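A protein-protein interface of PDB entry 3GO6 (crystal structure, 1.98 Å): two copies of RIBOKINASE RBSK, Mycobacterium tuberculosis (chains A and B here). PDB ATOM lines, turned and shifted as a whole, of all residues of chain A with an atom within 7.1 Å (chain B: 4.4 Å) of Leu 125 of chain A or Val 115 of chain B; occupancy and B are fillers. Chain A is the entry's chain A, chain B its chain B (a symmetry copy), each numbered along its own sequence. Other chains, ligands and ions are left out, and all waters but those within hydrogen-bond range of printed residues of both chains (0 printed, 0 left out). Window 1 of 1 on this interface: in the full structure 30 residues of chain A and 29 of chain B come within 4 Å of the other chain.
The side-chain hydroxyl (OG1) of Thr 123 of chain B sits at hydrogen-bond distance from the backbone NH (N) of Gly 43 of chain A.
N of Val 46 of chain B is in hydrogen-bond range of O of Val 124 of chain A (3.0 Å).
The backbone NH (N) of Val 126 of chain A lies within hydrogen-bond range of the backbone carbonyl oxygen (O) of Val 46 of chain B (2.9 Å).
The backbone carbonyl oxygen (O) of Val 126 of chain A sits at hydrogen-bond distance from the backbone NH (N) of Ala 48 of chain B, at 2.8 Å.
O of Thr 111 of chain A sits at hydrogen-bond distance from N of Ala 127 of chain A (2.8 Å).
The backbone carbonyl oxygen of Leu 125 of chain A lies within hydrogen-bond range of the backbone NH of Ile 113 of chain A (2.7 Å).
The backbone NH of Phe 34 of chain B is in hydrogen-bond range of the backbone carbonyl oxygen of Ile 114 of chain B.
O of Phe 34 of chain B sits at hydrogen-bond distance from N of Val 116 of chain B (2.9 Å).
O of Val 116 of chain B lies within hydrogen-bond range of N of Val 36 of chain B, at 2.9 Å.
O of Thr 123 of chain B is in hydrogen-bond range of N of Val 115 of chain B (2.8 Å).
Among the printed residues, pairs that only touch across the chains: Gly 43 of chain A with Glu 121 of chain B (3.4 Å), Gly 43 of chain A with Asn 122 of chain B (3.3 Å), Ile 113 of chain A with Phe 34 of chain B (3.4 Å), Ile 113 of chain A with Ile 113 of chain B (3.5 Å), Leu 125 of chain A with Phe 34 of chain B (3.7 Å), Leu 125 of chain A with Val 36 of chain B (3.4 Å), Leu 125 of chain A with Val 46 of chain B (3.4 Å), Leu 125 of chain A with Val 115 of chain B (3.8 Å) and Ala 127 of chain A with Phe 34 of chain B (3.7 Å).
Thr 123 of chain A touches none of the printed residues of chain B.
Of the printed residues of chain B, Val 124 of chain A touches Val 46 (3.0 Å).
Leu 125 of chain A touches just these residues of chain B: Phe 34 (3.7 Å), Val 36 (3.4 Å), Val 46 (3.4 Å) and Val 115 (3.8 Å).
Of the printed residues of chain A, Ala 48 of chain B touches Val 126.
Of chain A, only Leu 125 (3.8 Å) comes within 4 Å of Val 115 of chain B.
Val 116 of chain B touches none of the printed residues of chain A.
The nearest residue of chain A that does not touch Val 115 of chain B is Ile 113 of chain A (6.5 Å).
The nearest printed residue of chain B that does not touch Val 124 of chain A is Leu 39 of chain B (6.8 Å).
Of the 15 printed residues of chain A, 6 touch a printed residue of chain B.
Hydrophobic or aromatic side chains of chain A that line the printed part of chain B: Ile 113, Leu 125 and Ala 127.
Hydrophobic or aromatic side chains of chain B within 4 Å of the printed part of chain A: Phe 34, Val 36, Val 46, Ala 48, Ile 113 and Val 115.
Ile 113 of chain A touches its own counterpart, Ile 113 of chain B.
4 positions are printed for both chains.
Of the 13 pairs that touch across the chains among the printed residues, 1 has its exchanged pair printed and touching as well.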
ATOM      1  N   ASN A  29     -31.314  20.398  -3.115  1.00  0.00           N
ATOM      2  CA  ASN A  29     -30.079  20.260  -2.343  1.00  0.00           C
ATOM      3  C   ASN A  29     -29.663  18.811  -2.412  1.00  0.00           C
ATOM      4  O   ASN A  29     -30.521  17.940  -2.503  1.00  0.00           O
ATOM      5  CB  ASN A  29     -30.321  20.550  -0.835  1.00  0.00           C
ATOM      6  CG  ASN A  29     -30.835  21.949  -0.565  1.00  0.00           C
ATOM      7  OD1 ASN A  29     -30.363  22.915  -1.153  1.00  0.00           O
ATOM      8  ND2 ASN A  29     -31.823  22.063   0.339  1.00  0.00           N
ATOM      9  N   ASP A  31     -28.573  15.959   0.067  1.00  0.00           N
ATOM     10  CA  ASP A  31     -28.797  15.748   1.487  1.00  0.00           C
ATOM     11  C   ASP A  31     -27.797  14.751   2.027  1.00  0.00           C
ATOM     12  O   ASP A  31     -27.617  13.669   1.452  1.00  0.00           O
ATOM     13  CB  ASP A  31     -30.198  15.158   1.738  1.00  0.00           C
ATOM     14  CG  ASP A  31     -31.320  16.174   1.567  1.00  0.00           C
ATOM     15  OD1 ASP A  31     -31.030  17.386   1.475  1.00  0.00           O
ATOM     16  OD2 ASP A  31     -32.506  15.749   1.527  1.00  0.00           O
ATOM     17  N   LEU A  32     -27.188  15.101   3.150  1.00  0.00           N
ATOM     18  CA  LEU A  32     -26.363  14.160   3.914  1.00  0.00           C
ATOM     19  C   LEU A  32     -27.184  13.847   5.172  1.00  0.00           C
ATOM     20  O   LEU A  32     -27.411  14.726   5.988  1.00  0.00           O
ATOM     21  CB  LEU A  32     -25.018  14.782   4.267  1.00  0.00           C
ATOM     22  CG  LEU A  32     -24.141  15.134   3.048  1.00  0.00           C
ATOM     23  CD1 LEU A  32     -22.912  15.880   3.508  1.00  0.00           C
ATOM     24  CD2 LEU A  32     -23.735  13.889   2.278  1.00  0.00           C
ATOM     25  N   GLY A  43     -21.071  22.488  21.267  1.00  0.00           N
ATOM     26  CA  GLY A  43     -19.770  22.115  21.810  1.00  0.00           C
ATOM     27  C   GLY A  43     -19.457  20.637  21.786  1.00  0.00           C
ATOM     28  O   GLY A  43     -18.317  20.240  22.014  1.00  0.00           O
ATOM     29  N   THR A 111     -26.453  22.176  -0.300  1.00  0.00           N
ATOM     30  CA  THR A 111     -26.112  21.014   0.527  1.00  0.00           C
ATOM     31  C   THR A 111     -26.950  21.104   1.793  1.00  0.00           C
ATOM     32  O   THR A 111     -27.017  22.179   2.402  1.00  0.00           O
ATOM     33  CB  THR A 111     -24.600  21.018   0.956  1.00  0.00           C
ATOM     34  OG1 THR A 111     -23.746  21.015  -0.202  1.00  0.00           O
ATOM     35  CG2 THR A 111     -24.258  19.771   1.834  1.00  0.00           C
ATOM     36  N   ALA A 112     -27.578  20.006   2.201  1.00  0.00           N
ATOM     37  CA  ALA A 112     -28.254  20.010   3.501  1.00  0.00           C
ATOM     38  C   ALA A 112     -27.790  18.890   4.411  1.00  0.00           C
ATOM     39  O   ALA A 112     -27.458  17.800   3.934  1.00  0.00           O
ATOM     40  CB  ALA A 112     -29.750  19.938   3.320  1.00  0.00           C
ATOM     41  N   ILE A 113     -27.779  19.162   5.721  1.00  0.00           N
ATOM     42  CA  ILE A 113     -27.444  18.148   6.721  1.00  0.00           C
ATOM     43  C   ILE A 113     -28.734  17.816   7.469  1.00  0.00           C
ATOM     44  O   ILE A 113     -29.367  18.708   8.047  1.00  0.00           O
ATOM     45  CB  ILE A 113     -26.397  18.660   7.774  1.00  0.00           C
ATOM     46  CG1 ILE A 113     -25.152  19.243   7.093  1.00  0.00           C
ATOM     47  CG2 ILE A 113     -26.016  17.535   8.783  1.00  0.00           C
ATOM     48  CD1 ILE A 113     -24.469  18.279   6.111  1.00  0.00           C
ATOM     49  N   ILE A 114     -29.111  16.546   7.448  1.00  0.00           N
ATOM     50  CA  ILE A 114     -30.287  16.083   8.168  1.00  0.00           C
ATOM     51  C   ILE A 114     -29.784  15.152   9.272  1.00  0.00           C
ATOM     52  O   ILE A 114     -29.048  14.204   8.998  1.00  0.00           O
ATOM     53  CB  ILE A 114     -31.263  15.289   7.269  1.00  0.00           C
ATOM     54  CG1 ILE A 114     -31.434  15.916   5.859  1.00  0.00           C
ATOM     55  CG2 ILE A 114     -32.579  14.960   8.039  1.00  0.00           C
ATOM     56  CD1 ILE A 114     -32.124  17.132   5.831  1.00  0.00           C
ATOM     57  N   VAL A 115     -30.182  15.408  10.515  1.00  0.00           N
ATOM     58  CA  VAL A 115     -29.787  14.521  11.607  1.00  0.00           C
ATOM     59  C   VAL A 115     -31.061  13.933  12.231  1.00  0.00           C
ATOM     60  O   VAL A 115     -31.994  14.672  12.544  1.00  0.00           O
ATOM     61  CB  VAL A 115     -28.953  15.272  12.666  1.00  0.00           C
ATOM     62  CG1 VAL A 115     -28.358  14.270  13.698  1.00  0.00           C
ATOM     63  CG2 VAL A 115     -27.841  16.062  11.994  1.00  0.00           C
ATOM     64  N   THR A 123     -33.376  17.298  12.665  1.00  0.00           N
ATOM     65  CA  THR A 123     -33.003  18.699  12.458  1.00  0.00           C
ATOM     66  C   THR A 123     -32.484  18.829  11.040  1.00  0.00           C
ATOM     67  O   THR A 123     -31.957  17.852  10.471  1.00  0.00           O
ATOM     68  CB  THR A 123     -31.886  19.214  13.414  1.00  0.00           C
ATOM     69  OG1 THR A 123     -30.645  18.521  13.177  1.00  0.00           O
ATOM     70  CG2 THR A 123     -32.293  19.073  14.905  1.00  0.00           C
ATOM     71  N   VAL A 124     -32.627  20.025  10.474  1.00  0.00           N
ATOM     72  CA  VAL A 124     -32.165  20.260   9.097  1.00  0.00           C
ATOM     73  C   VAL A 124     -31.335  21.543   9.068  1.00  0.00           C
ATOM     74  O   VAL A 124     -31.770  22.579   9.601  1.00  0.00           O
ATOM     75  CB  VAL A 124     -33.363  20.349   8.113  1.00  0.00           C
ATOM     76  CG1 VAL A 124     -32.914  20.771   6.676  1.00  0.00           C
ATOM     77  CG2 VAL A 124     -34.126  19.032   8.051  1.00  0.00           C
ATOM     78  N   LEU A 125     -30.148  21.468   8.458  1.00  0.00           N
ATOM     79  CA  LEU A 125     -29.276  22.614   8.277  1.00  0.00           C
ATOM     80  C   LEU A 125     -28.907  22.702   6.797  1.00  0.00           C
ATOM     81  O   LEU A 125     -28.409  21.719   6.227  1.00  0.00           O
ATOM     82  CB  LEU A 125     -27.981  22.422   9.085  1.00  0.00           C
ATOM     83  CG  LEU A 125     -26.851  23.429   8.899  1.00  0.00           C
ATOM     84  CD1 LEU A 125     -27.279  24.810   9.325  1.00  0.00           C
ATOM     85  CD2 LEU A 125     -25.579  22.997   9.660  1.00  0.00           C
ATOM     86  N   VAL A 126     -29.088  23.881   6.198  1.00  0.00           N
ATOM     87  CA  VAL A 126     -28.981  24.018   4.732  1.00  0.00           C
ATOM     88  C   VAL A 126     -27.967  25.092   4.375  1.00  0.00           C
ATOM     89  O   VAL A 126     -28.042  26.214   4.879  1.00  0.00           O
ATOM     90  CB  VAL A 126     -30.338  24.417   4.087  1.00  0.00           C
ATOM     91  CG1 VAL A 126     -30.194  24.558   2.560  1.00  0.00           C
ATOM     92  CG2 VAL A 126     -31.445  23.399   4.442  1.00  0.00           C
ATOM     93  N   ALA A 127     -27.017  24.750   3.510  1.00  0.00           N
ATOM     94  CA  ALA A 127     -26.185  25.767   2.884  1.00  0.00           C
ATOM     95  C   ALA A 127     -26.782  25.869   1.480  1.00  0.00           C
ATOM     96  O   ALA A 127     -26.591  24.964   0.653  1.00  0.00           O
ATOM     97  CB  ALA A 127     -24.751  25.309   2.840  1.00  0.00           C
ATOM     98  N   GLU A 152     -36.213  28.754   1.078  1.00  0.00           N
ATOM     99  CA  GLU A 152     -34.749  28.585   0.977  1.00  0.00           C
ATOM    100  C   GLU A 152     -34.177  29.375  -0.210  1.00  0.00           C
ATOM    101  O   GLU A 152     -32.998  29.757  -0.209  1.00  0.00           O
ATOM    102  CB  GLU A 152     -34.339  27.110   0.865  1.00  0.00           C
ATOM    103  CG  GLU A 152     -34.828  26.212   2.032  1.00  0.00           C
ATOM    104  CD  GLU A 152     -34.323  24.759   1.895  1.00  0.00           C
ATOM    105  OE1 GLU A 152     -33.758  24.389   0.823  1.00  0.00           O
ATOM    106  OE2 GLU A 152     -34.459  23.997   2.872  1.00  0.00           O
ATOM    107  N   PHE B  34     -19.847  24.658   8.539  1.00  0.00           N
ATOM    108  CA  PHE B  34     -21.014  25.520   8.364  1.00  0.00           C
ATOM    109  C   PHE B  34     -20.950  26.634   9.413  1.00  0.00           C
ATOM    110  O   PHE B  34     -20.755  26.351  10.606  1.00  0.00           O
ATOM    111  CB  PHE B  34     -22.314  24.730   8.614  1.00  0.00           C
ATOM    112  CG  PHE B  34     -22.634  23.678   7.565  1.00  0.00           C
ATOM    113  CD1 PHE B  34     -23.557  23.943   6.558  1.00  0.00           C
ATOM    114  CD2 PHE B  34     -22.050  22.407   7.626  1.00  0.00           C
ATOM    115  CE1 PHE B  34     -23.884  22.964   5.596  1.00  0.00           C
ATOM    116  CE2 PHE B  34     -22.356  21.421   6.665  1.00  0.00           C
ATOM    117  CZ  PHE B  34     -23.283  21.698   5.654  1.00  0.00           C
ATOM    118  N   VAL B  36     -23.266  29.268  11.334  1.00  0.00           N
ATOM    119  CA  VAL B  36     -24.691  29.529  11.599  1.00  0.00           C
ATOM    120  C   VAL B  36     -24.860  30.497  12.783  1.00  0.00           C
ATOM    121  O   VAL B  36     -23.914  30.745  13.528  1.00  0.00           O
ATOM    122  CB  VAL B  36     -25.486  28.238  11.963  1.00  0.00           C
ATOM    123  CG1 VAL B  36     -25.301  27.135  10.907  1.00  0.00           C
ATOM    124  CG2 VAL B  36     -25.089  27.723  13.338  1.00  0.00           C
ATOM    125  N   LEU B  39     -27.537  26.354  16.186  1.00  0.00           N
ATOM    126  CA  LEU B  39     -27.909  25.014  15.750  1.00  0.00           C
ATOM    127  C   LEU B  39     -29.427  24.917  15.565  1.00  0.00           C
ATOM    128  O   LEU B  39     -30.177  25.556  16.301  1.00  0.00           O
ATOM    129  CB  LEU B  39     -27.462  23.962  16.767  1.00  0.00           C
ATOM    130  CG  LEU B  39     -25.992  23.528  16.826  1.00  0.00           C
ATOM    131  CD1 LEU B  39     -25.805  22.637  18.053  1.00  0.00           C
ATOM    132  CD2 LEU B  39     -25.537  22.782  15.558  1.00  0.00           C
ATOM    133  N   VAL B  46     -32.721  25.429   9.560  1.00  0.00           N
ATOM    134  CA  VAL B  46     -31.906  26.621   9.687  1.00  0.00           C
ATOM    135  C   VAL B  46     -31.063  26.768   8.403  1.00  0.00           C
ATOM    136  O   VAL B  46     -30.611  25.759   7.846  1.00  0.00           O
ATOM    137  CB  VAL B  46     -31.032  26.481  10.985  1.00  0.00           C
ATOM    138  CG1 VAL B  46     -29.725  27.228  10.922  1.00  0.00           C
ATOM    139  CG2 VAL B  46     -31.856  26.889  12.209  1.00  0.00           C
ATOM    140  N   ALA B  48     -27.492  28.096   6.842  1.00  0.00           N
ATOM    141  CA  ALA B  48     -26.112  28.486   7.162  1.00  0.00           C
ATOM    142  C   ALA B  48     -25.720  29.737   6.385  1.00  0.00           C
ATOM    143  O   ALA B  48     -26.152  29.914   5.240  1.00  0.00           O
ATOM    144  CB  ALA B  48     -25.124  27.334   6.834  1.00  0.00           C
ATOM    145  N   ILE B 113     -19.003  17.012   9.963  1.00  0.00           N
ATOM    146  CA  ILE B 113     -19.762  18.255   9.916  1.00  0.00           C
ATOM    147  C   ILE B 113     -19.325  19.067  11.123  1.00  0.00           C
ATOM    148  O   ILE B 113     -19.415  18.585  12.260  1.00  0.00           O
ATOM    149  CB  ILE B 113     -21.299  18.025  10.000  1.00  0.00           C
ATOM    150  CG1 ILE B 113     -21.799  16.989   8.987  1.00  0.00           C
ATOM    151  CG2 ILE B 113     -22.093  19.364   9.884  1.00  0.00           C
ATOM    152  CD1 ILE B 113     -21.398  17.217   7.524  1.00  0.00           C
ATOM    153  N   ILE B 114     -18.830  20.276  10.878  1.00  0.00           N
ATOM    154  CA  ILE B 114     -18.419  21.193  11.944  1.00  0.00           C
ATOM    155  C   ILE B 114     -19.295  22.414  11.836  1.00  0.00           C
ATOM    156  O   ILE B 114     -19.269  23.132  10.827  1.00  0.00           O
ATOM    157  CB  ILE B 114     -16.945  21.629  11.813  1.00  0.00           C
ATOM    158  CG1 ILE B 114     -16.006  20.426  11.869  1.00  0.00           C
ATOM    159  CG2 ILE B 114     -16.568  22.644  12.919  1.00  0.00           C
ATOM    160  CD1 ILE B 114     -15.474  19.959  10.521  1.00  0.00           C
ATOM    161  N   VAL B 115     -20.104  22.631  12.857  1.00  0.00           N
ATOM    162  CA  VAL B 115     -20.987  23.779  12.882  1.00  0.00           C
ATOM    163  C   VAL B 115     -20.444  24.788  13.881  1.00  0.00           C
ATOM    164  O   VAL B 115     -20.256  24.466  15.063  1.00  0.00           O
ATOM    165  CB  VAL B 115     -22.415  23.390  13.276  1.00  0.00           C
ATOM    166  CG1 VAL B 115     -23.313  24.635  13.264  1.00  0.00           C
ATOM    167  CG2 VAL B 115     -22.970  22.307  12.334  1.00  0.00           C
ATOM    168  N   VAL B 116     -20.191  26.001  13.397  1.00  0.00           N
ATOM    169  CA  VAL B 116     -19.675  27.093  14.207  1.00  0.00           C
ATOM    170  C   VAL B 116     -20.798  28.110  14.382  1.00  0.00           C
ATOM    171  O   VAL B 116     -21.273  28.690  13.405  1.00  0.00           O
ATOM    172  CB  VAL B 116     -18.467  27.777  13.521  1.00  0.00           C
ATOM    173  CG1 VAL B 116     -17.851  28.864  14.442  1.00  0.00           C
ATOM    174  CG2 VAL B 116     -17.411  26.750  13.119  1.00  0.00           C
ATOM    175  N   ASP B 117     -21.214  28.329  15.629  1.00  0.00           N
ATOM    176  CA  ASP B 117     -22.366  29.181  15.918  1.00  0.00           C
ATOM    177  C   ASP B 117     -21.980  30.579  16.418  1.00  0.00           C
ATOM    178  O   ASP B 117     -20.799  30.887  16.544  1.00  0.00           O
ATOM    179  CB  ASP B 117     -23.358  28.468  16.861  1.00  0.00           C
ATOM    180  CG  ASP B 117     -22.796  28.229  18.253  1.00  0.00           C
ATOM    181  OD1 ASP B 117     -22.005  29.069  18.747  1.00  0.00           O
ATOM    182  OD2 ASP B 117     -23.160  27.195  18.857  1.00  0.00           O
ATOM    183  N   GLU B 121     -19.094  28.334  19.660  1.00  0.00           N
ATOM    184  CA  GLU B 121     -19.018  26.908  19.985  1.00  0.00           C
ATOM    185  C   GLU B 121     -18.910  26.105  18.685  1.00  0.00           C
ATOM    186  O   GLU B 121     -19.565  26.437  17.686  1.00  0.00           O
ATOM    187  CB  GLU B 121     -20.254  26.429  20.755  1.00  0.00           C
ATOM    188  CG  GLU B 121     -20.457  27.027  22.141  1.00  0.00           C
ATOM    189  CD  GLU B 121     -19.601  26.370  23.210  1.00  0.00           C
ATOM    190  OE1 GLU B 121     -19.606  25.118  23.316  1.00  0.00           O
ATOM    191  OE2 GLU B 121     -18.924  27.119  23.959  1.00  0.00           O
ATOM    192  N   ASN B 122     -18.081  25.067  18.708  1.00  0.00           N
ATOM    193  CA  ASN B 122     -17.964  24.122  17.600  1.00  0.00           C
ATOM    194  C   ASN B 122     -18.653  22.826  17.928  1.00  0.00           C
ATOM    195  O   ASN B 122     -18.275  22.152  18.890  1.00  0.00           O
ATOM    196  CB  ASN B 122     -16.501  23.834  17.275  1.00  0.00           C
ATOM    197  CG  ASN B 122     -15.917  24.841  16.331  1.00  0.00           C
ATOM    198  OD1 ASN B 122     -16.240  26.028  16.395  1.00  0.00           O
ATOM    199  ND2 ASN B 122     -15.051  24.379  15.439  1.00  0.00           N
ATOM    200  N   THR B 123     -19.667  22.492  17.133  1.00  0.00           N
ATOM    201  CA  THR B 123     -20.418  21.257  17.280  1.00  0.00           C
ATOM    202  C   THR B 123     -20.073  20.353  16.126  1.00  0.00           C
ATOM    203  O   THR B 123     -20.199  20.750  14.961  1.00  0.00           O
ATOM    204  CB  THR B 123     -21.919  21.528  17.278  1.00  0.00           C
ATOM    205  OG1 THR B 123     -22.207  22.535  18.253  1.00  0.00           O
ATOM    206  CG2 THR B 123     -22.693  20.277  17.617  1.00  0.00           C
